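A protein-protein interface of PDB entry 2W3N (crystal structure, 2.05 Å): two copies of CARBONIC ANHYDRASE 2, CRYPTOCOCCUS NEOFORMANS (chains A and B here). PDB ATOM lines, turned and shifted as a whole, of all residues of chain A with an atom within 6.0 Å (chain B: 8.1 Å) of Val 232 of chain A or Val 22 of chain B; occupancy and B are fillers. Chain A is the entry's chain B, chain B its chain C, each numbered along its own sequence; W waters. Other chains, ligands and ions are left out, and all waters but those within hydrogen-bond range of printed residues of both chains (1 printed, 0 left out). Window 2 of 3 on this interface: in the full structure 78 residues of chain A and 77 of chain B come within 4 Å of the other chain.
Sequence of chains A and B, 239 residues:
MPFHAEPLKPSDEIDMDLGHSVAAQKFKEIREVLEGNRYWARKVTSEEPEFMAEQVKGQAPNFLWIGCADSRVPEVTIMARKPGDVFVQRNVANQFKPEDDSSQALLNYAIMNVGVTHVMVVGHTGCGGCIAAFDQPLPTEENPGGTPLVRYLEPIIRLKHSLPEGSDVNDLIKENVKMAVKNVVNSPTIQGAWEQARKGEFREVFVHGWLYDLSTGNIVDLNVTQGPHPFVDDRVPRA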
ATOM      1  N   ASP A 221       7.178 -13.085 -19.996  1.00  0.00           N
ATOM      2  CA  ASP A 221       8.158 -13.184 -21.076  1.00  0.00           C
ATOM      3  C   ASP A 221       8.733 -14.589 -21.077  1.00  0.00           C
ATOM      4  O   ASP A 221       9.275 -15.033 -20.057  1.00  0.00           O
ATOM      5  CB  ASP A 221       9.269 -12.169 -20.847  1.00  0.00           C
ATOM      6  CG  ASP A 221      10.158 -11.942 -22.083  1.00  0.00           C
ATOM      7  OD1 ASP A 221      10.131 -12.740 -23.032  1.00  0.00           O
ATOM      8  OD2 ASP A 221      10.928 -10.960 -22.071  1.00  0.00           O
ATOM      9  N   ASN A 223      11.282 -15.338 -22.695  1.00  0.00           N
ATOM     10  CA  ASN A 223      12.669 -15.088 -23.022  1.00  0.00           C
ATOM     11  C   ASN A 223      13.206 -15.844 -24.206  1.00  0.00           C
ATOM     12  O   ASN A 223      14.142 -16.658 -24.088  1.00  0.00           O
ATOM     13  CB  ASN A 223      13.570 -15.293 -21.779  1.00  0.00           C
ATOM     14  CG  ASN A 223      13.239 -14.332 -20.683  1.00  0.00           C
ATOM     15  OD1 ASN A 223      12.909 -14.732 -19.567  1.00  0.00           O
ATOM     16  ND2 ASN A 223      13.301 -13.048 -20.993  1.00  0.00           N
ATOM     17  N   PRO A 230      23.279 -11.439 -31.490  1.00  0.00           N
ATOM     18  CA  PRO A 230      23.202 -12.247 -30.260  1.00  0.00           C
ATOM     19  C   PRO A 230      22.651 -11.451 -29.066  1.00  0.00           C
ATOM     20  O   PRO A 230      23.171 -10.394 -28.702  1.00  0.00           O
ATOM     21  CB  PRO A 230      24.656 -12.677 -30.039  1.00  0.00           C
ATOM     22  CG  PRO A 230      25.190 -12.842 -31.468  1.00  0.00           C
ATOM     23  CD  PRO A 230      24.517 -11.718 -32.252  1.00  0.00           C
ATOM     24  N   PHE A 231      21.560 -11.961 -28.509  1.00  0.00           N
ATOM     25  CA  PHE A 231      20.728 -11.231 -27.565  1.00  0.00           C
ATOM     26  C   PHE A 231      20.897 -11.931 -26.237  1.00  0.00           C
ATOM     27  O   PHE A 231      20.247 -12.945 -25.977  1.00  0.00           O
ATOM     28  CB  PHE A 231      19.251 -11.279 -27.981  1.00  0.00           C
ATOM     29  CG  PHE A 231      18.362 -10.405 -27.141  1.00  0.00           C
ATOM     30  CD1 PHE A 231      18.086  -9.104 -27.526  1.00  0.00           C
ATOM     31  CD2 PHE A 231      17.818 -10.884 -25.946  1.00  0.00           C
ATOM     32  CE1 PHE A 231      17.295  -8.296 -26.734  1.00  0.00           C
ATOM     33  CE2 PHE A 231      17.006 -10.107 -25.167  1.00  0.00           C
ATOM     34  CZ  PHE A 231      16.744  -8.807 -25.542  1.00  0.00           C
ATOM     35  N   VAL A 232      21.783 -11.403 -25.404  1.00  0.00           N
ATOM     36  CA  VAL A 232      22.197 -12.117 -24.192  1.00  0.00           C
ATOM     37  C   VAL A 232      21.905 -11.316 -22.902  1.00  0.00           C
ATOM     38  O   VAL A 232      21.202 -11.814 -22.012  1.00  0.00           O
ATOM     39  CB  VAL A 232      23.691 -12.591 -24.308  1.00  0.00           C
ATOM     40  CG1 VAL A 232      24.174 -13.238 -23.020  1.00  0.00           C
ATOM     41  CG2 VAL A 232      23.842 -13.574 -25.480  1.00  0.00           C
ATOM     42  N   ASP A 233      22.394 -10.070 -22.849  1.00  0.00           N
ATOM     43  CA  ASP A 233      22.671  -9.325 -21.594  1.00  0.00           C
ATOM     44  C   ASP A 233      23.880  -9.887 -20.849  1.00  0.00           C
ATOM     45  O   ASP A 233      23.731 -10.484 -19.781  1.00  0.00           O
ATOM     46  CB  ASP A 233      21.457  -9.246 -20.644  1.00  0.00           C
ATOM     47  CG  ASP A 233      21.557  -8.072 -19.643  1.00  0.00           C
ATOM     48  OD1 ASP A 233      22.685  -7.611 -19.349  1.00  0.00           O
ATOM     49  OD2 ASP A 233      20.507  -7.596 -19.151  1.00  0.00           O
ATOM     50  N   LEU B  18       9.262  -8.264 -12.885  1.00  0.00           N
ATOM     51  CA  LEU B  18       9.699  -8.085 -14.267  1.00  0.00           C
ATOM     52  C   LEU B  18      11.167  -8.490 -14.480  1.00  0.00           C
ATOM     53  O   LEU B  18      11.672  -8.489 -15.610  1.00  0.00           O
ATOM     54  CB  LEU B  18       9.514  -6.633 -14.668  1.00  0.00           C
ATOM     55  CG  LEU B  18       8.050  -6.185 -14.805  1.00  0.00           C
ATOM     56  CD1 LEU B  18       8.044  -4.797 -15.403  1.00  0.00           C
ATOM     57  CD2 LEU B  18       7.204  -7.193 -15.602  1.00  0.00           C
ATOM     58  N   GLY B  19      11.846  -8.809 -13.384  1.00  0.00           N
ATOM     59  CA  GLY B  19      13.221  -9.278 -13.445  1.00  0.00           C
ATOM     60  C   GLY B  19      13.367 -10.524 -14.284  1.00  0.00           C
ATOM     61  O   GLY B  19      14.438 -10.758 -14.816  1.00  0.00           O
ATOM     62  N   HIS B  20      12.299 -11.303 -14.439  1.00  0.00           N
ATOM     63  CA  HIS B  20      12.350 -12.530 -15.251  1.00  0.00           C
ATOM     64  C   HIS B  20      12.576 -12.235 -16.747  1.00  0.00           C
ATOM     65  O   HIS B  20      13.099 -13.072 -17.494  1.00  0.00           O
ATOM     66  CB  HIS B  20      11.065 -13.339 -15.074  1.00  0.00           C
ATOM     67  CG  HIS B  20       9.886 -12.785 -15.825  1.00  0.00           C
ATOM     68  ND1 HIS B  20       9.152 -11.713 -15.373  1.00  0.00           N
ATOM     69  CD2 HIS B  20       9.308 -13.165 -16.995  1.00  0.00           C
ATOM     70  CE1 HIS B  20       8.180 -11.446 -16.229  1.00  0.00           C
ATOM     71  NE2 HIS B  20       8.247 -12.321 -17.218  1.00  0.00           N
ATOM     72  N   SER B  21      12.175 -11.041 -17.176  1.00  0.00           N
ATOM     73  CA  SER B  21      12.249 -10.660 -18.586  1.00  0.00           C
ATOM     74  C   SER B  21      13.558  -9.979 -18.910  1.00  0.00           C
ATOM     75  O   SER B  21      13.802  -8.839 -18.494  1.00  0.00           O
ATOM     76  CB  SER B  21      11.100  -9.734 -18.956  1.00  0.00           C
ATOM     77  OG  SER B  21      11.382  -9.067 -20.183  1.00  0.00           O
ATOM     78  N   VAL B  22      14.378 -10.670 -19.691  1.00  0.00           N
ATOM     79  CA  VAL B  22      15.590 -10.092 -20.254  1.00  0.00           C
ATOM     80  C   VAL B  22      15.281  -8.815 -21.016  1.00  0.00           C
ATOM     81  O   VAL B  22      15.930  -7.771 -20.815  1.00  0.00           O
ATOM     82  CB  VAL B  22      16.342 -11.125 -21.154  1.00  0.00           C
ATOM     83  CG1 VAL B  22      17.579 -10.499 -21.763  1.00  0.00           C
ATOM     84  CG2 VAL B  22      16.711 -12.395 -20.363  1.00  0.00           C
ATOM     85  N   ALA B  23      14.287  -8.859 -21.898  1.00  0.00           N
ATOM     86  CA  ALA B  23      14.031  -7.684 -22.754  1.00  0.00           C
ATOM     87  C   ALA B  23      13.575  -6.475 -21.969  1.00  0.00           C
ATOM     88  O   ALA B  23      13.939  -5.351 -22.310  1.00  0.00           O
ATOM     89  CB  ALA B  23      12.984  -8.029 -23.843  1.00  0.00           C
ATOM     90  N   ALA B  24      12.779  -6.682 -20.915  1.00  0.00           N
ATOM     91  CA  ALA B  24      12.383  -5.568 -20.023  1.00  0.00           C
ATOM     92  C   ALA B  24      13.570  -4.875 -19.369  1.00  0.00           C
ATOM     93  O   ALA B  24      13.482  -3.681 -19.006  1.00  0.00           O
ATOM     94  CB  ALA B  24      11.360  -6.045 -18.945  1.00  0.00           C
ATOM     95  N   GLN B  25      14.676  -5.605 -19.196  1.00  0.00           N
ATOM     96  CA  GLN B  25      15.913  -5.014 -18.705  1.00  0.00           C
ATOM     97  C   GLN B  25      16.617  -4.192 -19.791  1.00  0.00           C
ATOM     98  O   GLN B  25      17.353  -3.282 -19.465  1.00  0.00           O
ATOM     99  CB  GLN B  25      16.881  -6.052 -18.089  1.00  0.00           C
ATOM    100  CG  GLN B  25      16.276  -7.074 -17.078  1.00  0.00           C
ATOM    101  CD  GLN B  25      15.216  -6.487 -16.153  1.00  0.00           C
ATOM    102  OE1 GLN B  25      15.432  -5.455 -15.515  1.00  0.00           O
ATOM    103  NE2 GLN B  25      14.047  -7.152 -16.081  1.00  0.00           N
ATOM    104  N   LYS B  26      16.366  -4.492 -21.064  1.00  0.00           N
ATOM    105  CA  LYS B  26      17.061  -3.827 -22.175  1.00  0.00           C
ATOM    106  C   LYS B  26      16.297  -2.681 -22.866  1.00  0.00           C
ATOM    107  O   LYS B  26      16.916  -1.777 -23.465  1.00  0.00           O
ATOM    108  CB  LYS B  26      17.519  -4.857 -23.236  1.00  0.00           C
ATOM    109  CG  LYS B  26      18.185  -6.098 -22.650  1.00  0.00           C
ATOM    110  CD  LYS B  26      19.158  -6.767 -23.632  1.00  0.00           C
ATOM    111  N   PHE B  27      14.969  -2.734 -22.843  1.00  0.00           N
ATOM    112  CA  PHE B  27      14.180  -1.753 -23.558  1.00  0.00           C
ATOM    113  C   PHE B  27      13.202  -1.114 -22.604  1.00  0.00           C
ATOM    114  O   PHE B  27      12.320  -1.806 -22.058  1.00  0.00           O
ATOM    115  CB  PHE B  27      13.401  -2.373 -24.739  1.00  0.00           C
ATOM    116  CG  PHE B  27      14.259  -3.156 -25.704  1.00  0.00           C
ATOM    117  CD1 PHE B  27      14.966  -2.512 -26.711  1.00  0.00           C
ATOM    118  CD2 PHE B  27      14.340  -4.540 -25.607  1.00  0.00           C
ATOM    119  CE1 PHE B  27      15.764  -3.256 -27.605  1.00  0.00           C
ATOM    120  CE2 PHE B  27      15.123  -5.291 -26.495  1.00  0.00           C
ATOM    121  CZ  PHE B  27      15.838  -4.652 -27.481  1.00  0.00           C
ATOM    122  N   ILE B  30       9.643  -1.799 -23.672  1.00  0.00           N
ATOM    123  CA  ILE B  30       9.104  -3.088 -23.260  1.00  0.00           C
ATOM    124  C   ILE B  30       8.729  -3.104 -21.757  1.00  0.00           C
ATOM    125  O   ILE B  30       7.659  -3.583 -21.392  1.00  0.00           O
ATOM    126  CB  ILE B  30      10.052  -4.253 -23.573  1.00  0.00           C
ATOM    127  CG1 ILE B  30      10.251  -4.413 -25.115  1.00  0.00           C
ATOM    128  CG2 ILE B  30       9.534  -5.567 -22.946  1.00  0.00           C
ATOM    129  CD1 ILE B  30       9.143  -5.220 -25.872  1.00  0.00           C
ATOM    130  N   LEU B  34       5.050  -3.842 -19.925  1.00  0.00           N
ATOM    131  CA  LEU B  34       4.888  -4.886 -18.912  1.00  0.00           C
ATOM    132  C   LEU B  34       4.529  -4.308 -17.545  1.00  0.00           C
ATOM    133  O   LEU B  34       3.797  -4.927 -16.807  1.00  0.00           O
ATOM    134  CB  LEU B  34       6.125  -5.784 -18.822  1.00  0.00           C
ATOM    135  CG  LEU B  34       6.506  -6.595 -20.067  1.00  0.00           C
ATOM    136  CD1 LEU B  34       7.867  -7.316 -19.840  1.00  0.00           C
ATOM    137  CD2 LEU B  34       5.406  -7.595 -20.455  1.00  0.00           C
HETATM  138  O   HOH W   1      13.386 -11.409 -23.177  1.00  0.00           O
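Of the printed residues of chain B, Asp 221 of chain A touches His 20 (3.1 Å), Ser 21 (2.7 Å) and Ala 23 (3.97 Å). Printed residues of chain B within 4 Å of Asn 223 of chain A: His 20, Ser 21 and Val 22. Of the printed residues of chain B, Phe 231 of chain A touches Val 22, Lys 26 and Phe 27. Of chain B, only Val 22 comes within 4 Å of Val 232 of chain A. Of the printed residues of chain A, Ala 23 of chain B touches Asp 221 (3.97 Å). The nearest printed residue of chain A that does not touch Val 22 of chain B is Asp 221 of chain A (4.2 Å). The nearest printed residue of chain B that does not touch Asp 221 of chain A is Val 22 of chain B (4.2 Å).
Among the printed residues, merely in contact across the chains: Phe 231 of chain A with Val 22 of chain B (3.5 Å), Asn 223 of chain A with Ser 21 of chain B (3.6 Å), Phe 231 of chain A with Lys 26 of chain B (3.7 Å), Phe 231 of chain A with Phe 27 of chain B (3.7 Å), Val 232 of chain A with Val 22 of chain B (3.9 Å) and Asp 221 of chain A with Ala 23 of chain B (3.97 Å).
Hydrophobic or aromatic side chains of chain A that line the printed part of chain B: Phe 231. Of the 12 printed residues of chain B, 6 touch a printed residue of chain A. Hydrophobic or aromatic side chains of chain B that line the printed part of chain A: His 20, Val 22, Ala 23 and Phe 27.
Water W1 lies within hydrogen-bond range of the side-chain amide nitrogen (ND2) of Asn 223 of chain A, the side-chain carboxylate (OD2) of Asp 221 of chain A and the backbone NH (N) of Ala 23 of chain B.
No position is printed for both chains. Of the 10 pairs that touch across the chains among the printed residues, none has its exchanged pair printed and touching as well.
OG of Ser 21 of chain B sits close to N of Ala 23 of chain B, at 3.4 Å. The side-chain amide nitrogen of Gln 25 of chain B sits at hydrogen-bond distance from the backbone carbonyl oxygen of Ser 21 of chain B. OG of Ser 21 of chain B lies within hydrogen-bond range of N of Ala 24 of chain B, 2.9 Å away. OD1 of Asp 221 of chain A sits at hydrogen-bond distance from N of Asn 223 of chain A (2.9 Å).
The backbone NH (N) of Asp 221 of chain A is in hydrogen-bond range of a ring nitrogen (NE2) of His 20 of chain B. The side-chain carboxylate of Asp 221 of chain A sits at hydrogen-bond distance from the side-chain hydroxyl of Ser 21 of chain B. O of His 20 of chain B lies close to OD1 of Asn 223 of chain A (2.7 Å). N of Val 22 of chain B lies close to ND2 of Asn 223 of chain A.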
